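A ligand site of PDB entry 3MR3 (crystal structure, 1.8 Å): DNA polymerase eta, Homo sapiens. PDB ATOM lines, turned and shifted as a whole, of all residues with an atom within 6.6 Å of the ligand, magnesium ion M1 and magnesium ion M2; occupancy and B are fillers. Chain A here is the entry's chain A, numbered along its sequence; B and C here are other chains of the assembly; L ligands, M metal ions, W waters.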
ATOM      1  N   VAL A  15     -10.546  15.883 -18.705  1.00  0.00           N
ATOM      2  CA  VAL A  15     -11.208  14.608 -18.664  1.00  0.00           C
ATOM      3  C   VAL A  15     -10.712  13.829 -17.460  1.00  0.00           C
ATOM      4  O   VAL A  15      -9.501  13.732 -17.291  1.00  0.00           O
ATOM      5  CB  VAL A  15     -10.885  13.795 -19.946  1.00  0.00           C
ATOM      6  CG1 VAL A  15     -11.516  12.407 -19.870  1.00  0.00           C
ATOM      7  CG2 VAL A  15     -11.374  14.542 -21.188  1.00  0.00           C
ATOM      8  N   ASP A  16     -11.631  13.375 -16.604  1.00  0.00           N
ATOM      9  CA  ASP A  16     -11.257  12.658 -15.402  1.00  0.00           C
ATOM     10  C   ASP A  16     -12.006  11.351 -15.295  1.00  0.00           C
ATOM     11  O   ASP A  16     -13.240  11.349 -15.339  1.00  0.00           O
ATOM     12  CB  ASP A  16     -11.552  13.527 -14.186  1.00  0.00           C
ATOM     13  CG  ASP A  16     -11.110  12.871 -12.897  1.00  0.00           C
ATOM     14  OD1 ASP A  16     -11.807  11.961 -12.410  1.00  0.00           O
ATOM     15  OD2 ASP A  16     -10.029  13.261 -12.380  1.00  0.00           O
ATOM     16  N   MET A  17     -11.291  10.242 -15.110  1.00  0.00           N
ATOM     17  CA  MET A  17     -11.916   8.929 -15.022  1.00  0.00           C
ATOM     18  C   MET A  17     -12.807   8.830 -13.799  1.00  0.00           C
ATOM     19  O   MET A  17     -12.499   9.357 -12.723  1.00  0.00           O
ATOM     20  CB  MET A  17     -10.858   7.832 -14.978  1.00  0.00           C
ATOM     21  CG  MET A  17      -9.803   7.931 -16.067  1.00  0.00           C
ATOM     22  SD  MET A  17     -10.495   7.950 -17.739  1.00  0.00           S
ATOM     23  CE  MET A  17     -11.426   6.416 -17.745  1.00  0.00           C
ATOM     24  N   ASP A  18     -13.906   8.102 -13.943  1.00  0.00           N
ATOM     25  CA  ASP A  18     -14.793   7.875 -12.826  1.00  0.00           C
ATOM     26  C   ASP A  18     -14.250   6.748 -11.942  1.00  0.00           C
ATOM     27  O   ASP A  18     -13.800   5.731 -12.486  1.00  0.00           O
ATOM     28  CB  ASP A  18     -16.198   7.522 -13.320  1.00  0.00           C
ATOM     29  CG  ASP A  18     -16.826   8.612 -14.178  1.00  0.00           C
ATOM     30  OD1 ASP A  18     -16.457   9.812 -14.036  1.00  0.00           O
ATOM     31  OD2 ASP A  18     -17.729   8.305 -14.991  1.00  0.00           O
ATOM     32  N   CYS A  19     -14.254   6.977 -10.622  1.00  0.00           N
ATOM     33  CA  CYS A  19     -13.742   5.977  -9.659  1.00  0.00           C
ATOM     34  C   CYS A  19     -12.731   5.058 -10.362  1.00  0.00           C
ATOM     35  O   CYS A  19     -12.867   3.830 -10.418  1.00  0.00           O
ATOM     36  CB  CYS A  19     -14.926   5.157  -9.095  1.00  0.00           C
ATOM     37  SG  CYS A  19     -16.006   4.309 -10.282  1.00  0.00           S
ATOM     38  N   PHE A  20     -11.655   5.677 -10.783  1.00  0.00           N
ATOM     39  CA  PHE A  20     -10.666   5.046 -11.650  1.00  0.00           C
ATOM     40  C   PHE A  20     -10.090   3.711 -11.172  1.00  0.00           C
ATOM     41  O   PHE A  20     -10.137   2.738 -11.933  1.00  0.00           O
ATOM     42  CB  PHE A  20      -9.550   6.016 -12.001  1.00  0.00           C
ATOM     43  CG  PHE A  20      -8.609   5.483 -13.005  1.00  0.00           C
ATOM     44  CD1 PHE A  20      -9.062   4.893 -14.173  1.00  0.00           C
ATOM     45  CD2 PHE A  20      -7.240   5.584 -12.792  1.00  0.00           C
ATOM     46  CE1 PHE A  20      -8.177   4.399 -15.115  1.00  0.00           C
ATOM     47  CE2 PHE A  20      -6.351   5.098 -13.730  1.00  0.00           C
ATOM     48  CZ  PHE A  20      -6.818   4.513 -14.896  1.00  0.00           C
ATOM     49  N   PHE A  21      -9.486   3.635  -9.998  1.00  0.00           N
ATOM     50  CA  PHE A  21      -8.895   2.377  -9.570  1.00  0.00           C
ATOM     51  C   PHE A  21      -9.938   1.273  -9.494  1.00  0.00           C
ATOM     52  O   PHE A  21      -9.669   0.125  -9.835  1.00  0.00           O
ATOM     53  CB  PHE A  21      -8.175   2.520  -8.235  1.00  0.00           C
ATOM     54  CG  PHE A  21      -6.859   3.227  -8.330  1.00  0.00           C
ATOM     55  CD1 PHE A  21      -6.567   4.030  -9.434  1.00  0.00           C
ATOM     56  CD2 PHE A  21      -5.919   3.130  -7.319  1.00  0.00           C
ATOM     57  CE1 PHE A  21      -5.369   4.721  -9.519  1.00  0.00           C
ATOM     58  CE2 PHE A  21      -4.714   3.816  -7.399  1.00  0.00           C
ATOM     59  CZ  PHE A  21      -4.440   4.609  -8.492  1.00  0.00           C
ATOM     60  N   VAL A  22     -11.146   1.630  -9.076  1.00  0.00           N
ATOM     61  CA  VAL A  22     -12.246   0.676  -9.043  1.00  0.00           C
ATOM     62  C   VAL A  22     -12.591   0.162 -10.435  1.00  0.00           C
ATOM     63  O   VAL A  22     -12.750  -1.023 -10.637  1.00  0.00           O
ATOM     64  CB  VAL A  22     -13.503   1.314  -8.382  1.00  0.00           C
ATOM     65  CG1 VAL A  22     -14.722   0.453  -8.640  1.00  0.00           C
ATOM     66  CG2 VAL A  22     -13.292   1.500  -6.884  1.00  0.00           C
ATOM     67  N   GLN A  41      -5.573  -0.520   0.208  1.00  0.00           N
ATOM     68  CA  GLN A  41      -4.150  -0.847   0.213  1.00  0.00           C
ATOM     69  C   GLN A  41      -3.733  -1.285   1.608  1.00  0.00           C
ATOM     70  O   GLN A  41      -4.038  -0.596   2.616  1.00  0.00           O
ATOM     71  CB  GLN A  41      -3.225   0.262  -0.342  1.00  0.00           C
ATOM     72  CG  GLN A  41      -3.374   1.611   0.316  1.00  0.00           C
ATOM     73  CD  GLN A  41      -2.595   2.666  -0.444  1.00  0.00           C
ATOM     74  OE1 GLN A  41      -2.015   2.391  -1.512  1.00  0.00           O
ATOM     75  NE2 GLN A  41      -2.569   3.868   0.078  1.00  0.00           N
ATOM     76  N   ILE A  51      -8.812   3.788  -0.981  1.00  0.00           N
ATOM     77  CA  ILE A  51      -8.303   4.854  -1.835  1.00  0.00           C
ATOM     78  C   ILE A  51      -9.207   5.139  -3.046  1.00  0.00           C
ATOM     79  O   ILE A  51      -9.007   6.143  -3.704  1.00  0.00           O
ATOM     80  CB  ILE A  51      -6.835   4.627  -2.296  1.00  0.00           C
ATOM     81  CG1 ILE A  51      -6.663   3.303  -3.027  1.00  0.00           C
ATOM     82  CG2 ILE A  51      -5.891   4.698  -1.099  1.00  0.00           C
ATOM     83  CD1 ILE A  51      -5.323   3.242  -3.753  1.00  0.00           C
ATOM     84  N   ALA A  52     -10.178   4.279  -3.314  1.00  0.00           N
ATOM     85  CA  ALA A  52     -11.118   4.489  -4.413  1.00  0.00           C
ATOM     86  C   ALA A  52     -12.455   3.809  -4.112  1.00  0.00           C
ATOM     87  O   ALA A  52     -12.477   2.709  -3.598  1.00  0.00           O
ATOM     88  CB  ALA A  52     -10.540   4.031  -5.737  1.00  0.00           C
ATOM     89  N   VAL A  53     -13.553   4.460  -4.473  1.00  0.00           N
ATOM     90  CA  VAL A  53     -14.902   3.969  -4.139  1.00  0.00           C
ATOM     91  C   VAL A  53     -15.873   4.071  -5.306  1.00  0.00           C
ATOM     92  O   VAL A  53     -16.002   5.130  -5.902  1.00  0.00           O
ATOM     93  CB  VAL A  53     -15.457   4.816  -2.955  1.00  0.00           C
ATOM     94  CG1 VAL A  53     -16.728   4.207  -2.415  1.00  0.00           C
ATOM     95  CG2 VAL A  53     -14.407   4.963  -1.857  1.00  0.00           C
ATOM     96  N   TYR A  55     -19.464   4.439  -7.262  1.00  0.00           N
ATOM     97  CA  TYR A  55     -20.563   5.314  -6.959  1.00  0.00           C
ATOM     98  C   TYR A  55     -21.656   4.597  -6.171  1.00  0.00           C
ATOM     99  O   TYR A  55     -22.333   5.208  -5.351  1.00  0.00           O
ATOM    100  CB  TYR A  55     -21.126   5.962  -8.227  1.00  0.00           C
ATOM    101  CG  TYR A  55     -20.208   7.083  -8.676  1.00  0.00           C
ATOM    102  CD1 TYR A  55     -18.976   6.826  -9.272  1.00  0.00           C
ATOM    103  CD2 TYR A  55     -20.539   8.414  -8.394  1.00  0.00           C
ATOM    104  CE1 TYR A  55     -18.080   7.858  -9.568  1.00  0.00           C
ATOM    105  CE2 TYR A  55     -19.663   9.451  -8.681  1.00  0.00           C
ATOM    106  CZ  TYR A  55     -18.446   9.171  -9.266  1.00  0.00           C
ATOM    107  OH  TYR A  55     -17.610  10.221  -9.549  1.00  0.00           O
ATOM    108  N   ARG A  58     -20.556   4.827  -2.633  1.00  0.00           N
ATOM    109  CA  ARG A  58     -20.626   6.184  -2.108  1.00  0.00           C
ATOM    110  C   ARG A  58     -21.995   6.494  -1.557  1.00  0.00           C
ATOM    111  O   ARG A  58     -22.148   7.326  -0.654  1.00  0.00           O
ATOM    112  CB  ARG A  58     -20.252   7.211  -3.182  1.00  0.00           C
ATOM    113  CG  ARG A  58     -18.821   7.114  -3.640  1.00  0.00           C
ATOM    114  CD  ARG A  58     -18.498   8.146  -4.707  1.00  0.00           C
ATOM    115  NE  ARG A  58     -17.296   7.731  -5.417  1.00  0.00           N
ATOM    116  CZ  ARG A  58     -16.584   8.521  -6.208  1.00  0.00           C
ATOM    117  NH1 ARG A  58     -16.954   9.780  -6.406  1.00  0.00           N
ATOM    118  NH2 ARG A  58     -15.508   8.040  -6.822  1.00  0.00           N
ATOM    119  N   ARG A  64     -12.931   7.698   0.622  1.00  0.00           N
ATOM    120  CA  ARG A  64     -11.504   7.577   0.636  1.00  0.00           C
ATOM    121  C   ARG A  64     -10.989   8.044   2.007  1.00  0.00           C
ATOM    122  O   ARG A  64     -11.741   8.739   2.690  1.00  0.00           O
ATOM    123  CB  ARG A  64     -10.998   8.463  -0.504  1.00  0.00           C
ATOM    124  CG  ARG A  64      -9.576   8.985  -0.398  1.00  0.00           C
ATOM    125  CD  ARG A  64      -9.321   9.742  -1.696  1.00  0.00           C
ATOM    126  NE  ARG A  64      -9.731   8.923  -2.842  1.00  0.00           N
ATOM    127  CZ  ARG A  64     -10.012   9.396  -4.057  1.00  0.00           C
ATOM    128  NH1 ARG A  64      -9.938  10.691  -4.308  1.00  0.00           N
ATOM    129  NH2 ARG A  64     -10.370   8.560  -5.013  1.00  0.00           N
ATOM    130  N   LEU A  92       1.627   0.273  -7.748  1.00  0.00           N
ATOM    131  CA  LEU A  92       0.537   0.839  -8.528  1.00  0.00           C
ATOM    132  C   LEU A  92       0.673   0.653 -10.024  1.00  0.00           C
ATOM    133  O   LEU A  92       0.003   1.322 -10.804  1.00  0.00           O
ATOM    134  CB  LEU A  92       0.425   2.326  -8.187  1.00  0.00           C
ATOM    135  CG  LEU A  92       0.300   2.651  -6.697  1.00  0.00           C
ATOM    136  CD1 LEU A  92       0.271   4.154  -6.484  1.00  0.00           C
ATOM    137  CD2 LEU A  92      -0.940   2.010  -6.115  1.00  0.00           C
ATOM    138  N   SER A 116      -2.843  14.049 -13.632  1.00  0.00           N
ATOM    139  CA  SER A 116      -2.855  13.062 -12.551  1.00  0.00           C
ATOM    140  C   SER A 116      -2.849  11.681 -13.169  1.00  0.00           C
ATOM    141  O   SER A 116      -2.843  11.558 -14.393  1.00  0.00           O
ATOM    142  CB  SER A 116      -4.086  13.209 -11.654  1.00  0.00           C
ATOM    143  OG  SER A 116      -5.233  12.631 -12.239  1.00  0.00           O
ATOM    144  N   ILE A 117      -2.855  10.626 -12.368  1.00  0.00           N
ATOM    145  CA  ILE A 117      -2.887   9.287 -12.922  1.00  0.00           C
ATOM    146  C   ILE A 117      -4.190   9.075 -13.697  1.00  0.00           C
ATOM    147  O   ILE A 117      -4.256   8.268 -14.616  1.00  0.00           O
ATOM    148  CB  ILE A 117      -2.777   8.230 -11.796  1.00  0.00           C
ATOM    149  CG1 ILE A 117      -2.384   6.873 -12.398  1.00  0.00           C
ATOM    150  CG2 ILE A 117      -4.092   8.116 -11.047  1.00  0.00           C
ATOM    151  CD1 ILE A 117      -1.972   5.834 -11.341  1.00  0.00           C
ATOM    152  N   ASP A 118      -5.250   9.816 -13.368  1.00  0.00           N
ATOM    153  CA  ASP A 118      -6.544   9.613 -14.021  1.00  0.00           C
ATOM    154  C   ASP A 118      -7.131  10.822 -14.744  1.00  0.00           C
ATOM    155  O   ASP A 118      -8.306  10.798 -15.084  1.00  0.00           O
ATOM    156  CB  ASP A 118      -7.550   9.058 -13.006  1.00  0.00           C
ATOM    157  CG  ASP A 118      -8.415  10.098 -12.334  1.00  0.00           C
ATOM    158  OD1 ASP A 118      -9.629   9.859 -12.268  1.00  0.00           O
ATOM    159  OD2 ASP A 118      -7.906  11.153 -11.885  1.00  0.00           O
ATOM    160  N   GLU A 119      -6.388  11.873 -15.048  1.00  0.00           N
ATOM    161  CA  GLU A 119      -6.967  12.996 -15.771  1.00  0.00           C
ATOM    162  C   GLU A 119      -5.957  13.764 -16.595  1.00  0.00           C
ATOM    163  O   GLU A 119      -4.770  13.777 -16.315  1.00  0.00           O
ATOM    164  CB  GLU A 119      -7.691  13.942 -14.800  1.00  0.00           C
ATOM    165  CG  GLU A 119      -6.777  14.743 -13.892  1.00  0.00           C
ATOM    166  CD  GLU A 119      -7.413  15.059 -12.566  1.00  0.00           C
ATOM    167  OE1 GLU A 119      -7.909  16.185 -12.381  1.00  0.00           O
ATOM    168  OE2 GLU A 119      -7.428  14.171 -11.689  1.00  0.00           O
ATOM    169  N   SER A 216     -15.750  11.397 -16.994  1.00  0.00           N
ATOM    170  CA  SER A 216     -16.510  12.603 -17.074  1.00  0.00           C
ATOM    171  C   SER A 216     -15.622  13.697 -17.638  1.00  0.00           C
ATOM    172  O   SER A 216     -14.408  13.495 -17.743  1.00  0.00           O
ATOM    173  CB  SER A 216     -17.059  13.001 -15.698  1.00  0.00           C
ATOM    174  OG  SER A 216     -17.938  11.991 -15.243  1.00  0.00           O
ATOM    175  N   LYS A 234     -20.586  14.354 -12.487  1.00  0.00           N
ATOM    176  CA  LYS A 234     -20.094  12.989 -12.417  1.00  0.00           C
ATOM    177  C   LYS A 234     -21.187  12.101 -11.839  1.00  0.00           C
ATOM    178  O   LYS A 234     -21.945  12.533 -10.973  1.00  0.00           O
ATOM    179  CB  LYS A 234     -18.851  12.911 -11.528  1.00  0.00           C
ATOM    180  CG  LYS A 234     -17.551  13.207 -12.250  1.00  0.00           C
ATOM    181  CD  LYS A 234     -16.380  13.050 -11.285  1.00  0.00           C
ATOM    182  CE  LYS A 234     -15.060  13.006 -12.028  1.00  0.00           C
ATOM    183  NZ  LYS A 234     -14.761  11.653 -12.609  1.00  0.00           N
ATOM    184  N   PRO A 235     -21.228  10.823 -12.241  1.00  0.00           N
ATOM    185  CA  PRO A 235     -20.319  10.181 -13.188  1.00  0.00           C
ATOM    186  C   PRO A 235     -20.868  10.085 -14.616  1.00  0.00           C
ATOM    187  O   PRO A 235     -22.051  10.336 -14.884  1.00  0.00           O
ATOM    188  CB  PRO A 235     -20.167   8.779 -12.584  1.00  0.00           C
ATOM    189  CG  PRO A 235     -21.557   8.505 -12.076  1.00  0.00           C
ATOM    190  CD  PRO A 235     -22.027   9.821 -11.498  1.00  0.00           C
ATOM    191  P    DT B   9      -7.537  17.535  -6.514  1.00  0.00           P
ATOM    192  OP1  DT B   9      -8.701  17.939  -7.311  1.00  0.00           O
ATOM    193  OP2  DT B   9      -7.669  17.349  -5.033  1.00  0.00           O
ATOM    194  O5'  DT B   9      -6.904  16.204  -7.075  1.00  0.00           O
ATOM    195  C5'  DT B   9      -6.456  16.066  -8.415  1.00  0.00           C
ATOM    196  C4'  DT B   9      -5.994  14.639  -8.632  1.00  0.00           C
ATOM    197  O4'  DT B   9      -4.940  14.363  -7.666  1.00  0.00           O
ATOM    198  C3'  DT B   9      -7.110  13.625  -8.340  1.00  0.00           C
ATOM    199  O3'  DT B   9      -7.157  12.622  -9.356  1.00  0.00           O
ATOM    200  C2'  DT B   9      -6.728  13.014  -6.995  1.00  0.00           C
ATOM    201  C1'  DT B   9      -5.224  13.145  -6.955  1.00  0.00           C
ATOM    202  N1   DT B   9      -4.686  13.269  -5.576  1.00  0.00           N
ATOM    203  C2   DT B   9      -3.736  12.359  -5.117  1.00  0.00           C
ATOM    204  O2   DT B   9      -3.302  11.440  -5.780  1.00  0.00           O
ATOM    205  N3   DT B   9      -3.329  12.590  -3.828  1.00  0.00           N
ATOM    206  C4   DT B   9      -3.752  13.592  -2.978  1.00  0.00           C
ATOM    207  O4   DT B   9      -3.272  13.667  -1.843  1.00  0.00           O
ATOM    208  C5   DT B   9      -4.735  14.499  -3.527  1.00  0.00           C
ATOM    209  C7   DT B   9      -5.238  15.615  -2.676  1.00  0.00           C
ATOM    210  C6   DT B   9      -5.146  14.292  -4.789  1.00  0.00           C
ATOM    211  P   TTD C   3      -4.045   7.854  11.541  1.00  0.00           P
ATOM    212  OP1 TTD C   3      -5.512   7.710  11.325  1.00  0.00           O
ATOM    213  OP2 TTD C   3      -3.548   8.668  12.673  1.00  0.00           O
ATOM    214  O5' TTD C   3      -3.203   8.459  10.313  1.00  0.00           O
ATOM    215  C5' TTD C   3      -3.638   8.149   8.964  1.00  0.00           C
ATOM    216  C4R TTD C   3      -3.051   6.925   8.465  1.00  0.00           C
ATOM    217  O4' TTD C   3      -3.769   6.764   7.215  1.00  0.00           O
ATOM    218  C3R TTD C   3      -1.557   6.889   7.976  1.00  0.00           C
ATOM    219  O3R TTD C   3      -1.191   5.504   7.921  1.00  0.00           O
ATOM    220  C2' TTD C   3      -1.673   7.433   6.522  1.00  0.00           C
ATOM    221  C1' TTD C   3      -2.890   6.643   6.117  1.00  0.00           C
ATOM    222  N1  TTD C   3      -3.570   7.157   4.906  1.00  0.00           N
ATOM    223  C2  TTD C   3      -4.652   6.489   4.377  1.00  0.00           C
ATOM    224  O2  TTD C   3      -4.853   5.301   4.709  1.00  0.00           O
ATOM    225  N3  TTD C   3      -5.412   7.076   3.375  1.00  0.00           N
ATOM    226  C4  TTD C   3      -5.249   8.393   2.905  1.00  0.00           C
ATOM    227  O4  TTD C   3      -6.074   8.860   2.109  1.00  0.00           O
ATOM    228  C5  TTD C   3      -4.134   9.229   3.326  1.00  0.00           C
ATOM    229  C5A TTD C   3      -4.696  10.430   4.197  1.00  0.00           C
ATOM    230  C6  TTD C   3      -3.219   8.390   4.206  1.00  0.00           C
ATOM    231  PB  TTD C   3       0.166   5.031   7.302  1.00  0.00           P
ATOM    232  O5P TTD C   3       0.186   3.669   7.738  1.00  0.00           O
ATOM    233  O4P TTD C   3       1.261   6.007   7.646  1.00  0.00           O
ATOM    234  O5R TTD C   3      -0.042   5.108   5.745  1.00  0.00           O
ATOM    235  C5R TTD C   3      -0.580   4.008   5.095  1.00  0.00           C
ATOM    236  O4R TTD C   3      -1.581   5.474   3.400  1.00  0.00           O
ATOM    237  C2R TTD C   3       0.281   6.100   2.206  1.00  0.00           C
ATOM    238  C1R TTD C   3      -1.244   6.070   2.196  1.00  0.00           C
ATOM    239  N1T TTD C   3      -1.985   7.323   1.929  1.00  0.00           N
ATOM    240  C2T TTD C   3      -2.467   7.418   0.638  1.00  0.00           C
ATOM    241  O2T TTD C   3      -2.443   6.436  -0.139  1.00  0.00           O
ATOM    242  N3T TTD C   3      -3.094   8.575   0.278  1.00  0.00           N
ATOM    243  C4T TTD C   3      -3.140   9.625   1.178  1.00  0.00           C
ATOM    244  O4T TTD C   3      -3.551  10.737   0.731  1.00  0.00           O
ATOM    245  C5T TTD C   3      -2.799   9.566   2.587  1.00  0.00           C
ATOM    246  C5M TTD C   3      -2.038  10.799   3.116  1.00  0.00           C
ATOM    247  C6T TTD C   3      -2.074   8.237   3.099  1.00  0.00           C
ATOM    248  C4' TTD C   3      -0.680   4.355   3.597  1.00  0.00           C
ATOM    249  C3' TTD C   3       0.636   4.846   3.021  1.00  0.00           C
ATOM    250  O3' TTD C   3       1.060   3.887   2.105  1.00  0.00           O
ATOM    251  P    DA C   4       2.570   3.972   1.572  1.00  0.00           P
ATOM    252  OP1  DA C   4       3.101   2.592   1.567  1.00  0.00           O
ATOM    253  OP2  DA C   4       3.332   5.046   2.285  1.00  0.00           O
ATOM    254  O5'  DA C   4       2.354   4.478   0.086  1.00  0.00           O
ATOM    255  C5'  DA C   4       1.628   3.662  -0.849  1.00  0.00           C
ATOM    256  C4'  DA C   4       1.626   4.323  -2.198  1.00  0.00           C
ATOM    257  O4'  DA C   4       0.809   5.518  -2.207  1.00  0.00           O
ATOM    258  C3'  DA C   4       3.005   4.784  -2.644  1.00  0.00           C
ATOM    259  O3'  DA C   4       3.089   4.618  -4.063  1.00  0.00           O
ATOM    260  C2'  DA C   4       3.023   6.254  -2.303  1.00  0.00           C
ATOM    261  C1'  DA C   4       1.599   6.630  -2.628  1.00  0.00           C
ATOM    262  N9   DA C   4       1.093   7.807  -1.928  1.00  0.00           N
ATOM    263  C8   DA C   4       1.409   8.191  -0.660  1.00  0.00           C
ATOM    264  N7   DA C   4       0.794   9.280  -0.272  1.00  0.00           N
ATOM    265  C5   DA C   4       0.035   9.644  -1.376  1.00  0.00           C
ATOM    266  C6   DA C   4      -0.826  10.716  -1.608  1.00  0.00           C
ATOM    267  N6   DA C   4      -1.096  11.668  -0.711  1.00  0.00           N
ATOM    268  N1   DA C   4      -1.432  10.795  -2.812  1.00  0.00           N
ATOM    269  C2   DA C   4      -1.169   9.848  -3.715  1.00  0.00           C
ATOM    270  N3   DA C   4      -0.365   8.784  -3.623  1.00  0.00           N
ATOM    271  C4   DA C   4       0.212   8.744  -2.403  1.00  0.00           C
HETATM  272  N1  LIG L   1      -4.174   8.718  -2.184  1.00  0.00           N
HETATM  273  C1  LIG L   1      -3.934   7.668  -3.050  1.00  0.00           C
HETATM  274  N2  LIG L   1      -4.549   7.513  -4.128  1.00  0.00           N
HETATM  275  C2  LIG L   1      -5.440   8.469  -4.610  1.00  0.00           C
HETATM  276  C3  LIG L   1      -5.841   9.556  -3.759  1.00  0.00           C
HETATM  277  C4  LIG L   1      -5.044   9.721  -2.487  1.00  0.00           C
HETATM  278  N3  LIG L   1      -5.303  10.686  -1.747  1.00  0.00           N
HETATM  279  N4  LIG L   1      -6.688  10.266  -4.429  1.00  0.00           N
HETATM  280  C5  LIG L   1      -6.864   9.594  -5.487  1.00  0.00           C
HETATM  281  N5  LIG L   1      -6.173   8.527  -5.589  1.00  0.00           N
HETATM  282  P1  LIG L   1      -9.755  10.912  -8.458  1.00  0.00           P
HETATM  283  P2  LIG L   1     -11.788   8.691  -8.691  1.00  0.00           P
HETATM  284  P3  LIG L   1     -14.018  10.257  -9.393  1.00  0.00           P
HETATM  285  C6  LIG L   1      -6.123   7.579  -6.729  1.00  0.00           C
HETATM  286  O1  LIG L   1     -10.024  11.222  -9.592  1.00  0.00           O
HETATM  287  O2  LIG L   1     -11.347   8.657  -9.874  1.00  0.00           O
HETATM  288  O3  LIG L   1     -13.170  10.922 -10.063  1.00  0.00           O
HETATM  289  C7  LIG L   1      -7.297   6.550  -6.650  1.00  0.00           C
HETATM  290  O4  LIG L   1      -9.588  11.912  -7.437  1.00  0.00           O
HETATM  291  O5  LIG L   1     -11.608   7.629  -8.031  1.00  0.00           O
HETATM  292  O6  LIG L   1     -15.065   9.743 -10.098  1.00  0.00           O
HETATM  293  C8  LIG L   1      -8.351   7.075  -7.595  1.00  0.00           C
HETATM  294  O7  LIG L   1      -9.204   6.228  -8.139  1.00  0.00           O
HETATM  295  N6  LIG L   1     -10.918   9.920  -7.901  1.00  0.00           N
HETATM  296  O8  LIG L   1     -13.322   9.029  -8.649  1.00  0.00           O
HETATM  297  O9  LIG L   1     -14.553  10.972  -8.369  1.00  0.00           O
HETATM  298  C9  LIG L   1      -7.370   7.784  -8.565  1.00  0.00           C
HETATM  299  O10 LIG L   1      -6.281   8.199  -7.910  1.00  0.00           O
HETATM  300  C10 LIG L   1      -8.163   8.986  -9.224  1.00  0.00           C
HETATM  301  O11 LIG L   1      -8.439  10.112  -8.388  1.00  0.00           O
HETATM  302 MG    MG M   1     -11.389  10.337 -11.271  1.00  0.00          MG
HETATM  303 MG    MG M   2      -8.729  12.734 -10.900  1.00  0.00          MG
HETATM  304  O   HOH W   1      -9.757  14.170  -9.736  1.00  0.00           O
HETATM  305  O   HOH W   2      -5.399  10.744  -9.156  1.00  0.00           O
HETATM  306  O   HOH W   3     -10.329  14.295  -6.274  1.00  0.00           O
HETATM  307  O   HOH W   4      -7.396  12.588  -3.043  1.00  0.00           O
HETATM  308  O   HOH W   5     -13.336  11.417  -5.919  1.00  0.00           O
HETATM  309  O   HOH W   6     -13.043   6.973  -5.636  1.00  0.00           O
HETATM  310  O   HOH W   7      -2.742   5.640  -5.380  1.00  0.00           O
HETATM  311  O   HOH W   8     -12.593  13.575  -9.508  1.00  0.00           O
HETATM  312  O   HOH W   9     -15.850  13.290  -7.758  1.00  0.00           O
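Magnesium ion M2 is bound by OD2 of Asp 118, at 2.0 Å.
OD2 of Asp 16 is bound to magnesium ion M2 (2.0 Å).
Magnesium ion M2 is bound by the side-chain carboxylate (OE2) of Glu 119, at 2.1 Å.
Water W1 binds magnesium ion M2, at 2.1 Å.
O3' of DT 9 of chain B is bound to magnesium ion M2 (2.2 Å).
Magnesium ion M2 is bound by an oxygen (O1) of the ligand (2.4 Å).
The side-chain hydroxyl (OG) of Ser 116 is in hydrogen-bond range of the backbone NH (N) of Asp 118, at 3.0 Å.
NZ of Lys 234 sits close to O of Met 17 (3.2 Å).
The backbone NH of Glu 119 lies close to the side-chain hydroxyl of Ser 116 (3.1 Å).
The side-chain amide nitrogen (NE2) of Gln 41 sits at hydrogen-bond distance from O2T of TTD 3 of chain C (2.6 Å).
NE of Arg 58 sits at hydrogen-bond distance from O of Val 53 (2.9 Å).
OD1 of Asp 18 lies within salt-bridge range of NZ of Lys 234, 2.9 Å away.
The guanidinium group (NE) of Arg 64 is in hydrogen-bond range of the backbone carbonyl oxygen (O) of Ile 51.
OD1 of Asp 18 sits at hydrogen-bond distance from OG of Ser 216 (2.9 Å).
N3 of the ligand lies within hydrogen-bond range of N3 of DT 9 of chain B.
The side-chain hydroxyl of Tyr 55 lies within hydrogen-bond range of an oxygen (O6) of the ligand (2.6 Å).
A nitrogen (N3) of the ligand is in hydrogen-bond range of O4T of TTD 3 of chain C (3.0 Å).
The backbone NH (N) of Cys 19 lies within hydrogen-bond range of an oxygen (O6) of the ligand, 2.9 Å away.
The guanidinium group (NH1) of Arg 58 lies within salt-bridge range of an oxygen (O9) of the ligand (3.3 Å).
An oxygen (O6) of the ligand lies within salt-bridge range of the side-chain amino group of Lys 234, 3.2 Å away.
N of Phe 20 sits at hydrogen-bond distance from O5 of the ligand (3.4 Å).
N of Phe 21 is in hydrogen-bond range of O7 of the ligand (3.2 Å).
The guanidinium group (NH1) of Arg 64 is in salt-bridge range of an oxygen (O4) of the ligand (3.4 Å).
Merely in contact with magnesium ion M2: Ser 116 (3.7 Å).
Five residues have an atom within 4 Å of magnesium ion M2: Asp 16, Ser 116, Asp 118, Glu 119 and DT 9 of chain B.
Along chain A the residues within 4 Å of magnesium ion M2 span positions 16 to 119.
The nearest printed residue that does not touch magnesium ion M2 is Met 17 (5.4 Å).
Water W4 lies within hydrogen-bond range of a nitrogen (N4) of the ligand (2.8 Å) and the guanidinium group (NH1) of Arg 64 (3.4 Å).
N1 of DA 4 of chain C sits close to N1 of the ligand (3.5 Å).
Asp 18 touches the ligand.
O of Ile 51 touches C7 of the ligand, 3.4 Å away.
Ala 52 touches the ligand (CB to O7, 3.5 Å).
Ile 117 touches the ligand.
Hydrophobic or aromatic side chains that line the ligand: Phe 20, Phe 21, Ala 52, Tyr 55 and Ile 117.
Within 4 Å of the ligand: Asp 16, Met 17, Asp 18, Cys 19, Phe 20, Phe 21, Ile 51, Ala 52, Tyr 55, Arg 58, Arg 64, Ile 117, Asp 118, Lys 234, DT 9 of chain B, TTD 3 of chain C and DA 4 of chain C.
The nearest printed residue that does not touch the ligand is Glu 119 (4.5 Å).
NZ of Lys 234 touches magnesium ion M1, at 3.9 Å.
The nearest printed residue that does not touch magnesium ion M1 is Asp 18 (4.3 Å).
Magnesium ion M1 is bound by OD1 of Asp 16 (2.0 Å), O of Met 17 (2.1 Å), OD1 of Asp 118 (2.1 Å), O2 of the ligand (2.2 Å), O3 of the ligand (2.2 Å) and O1 of the ligand (2.3 Å).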
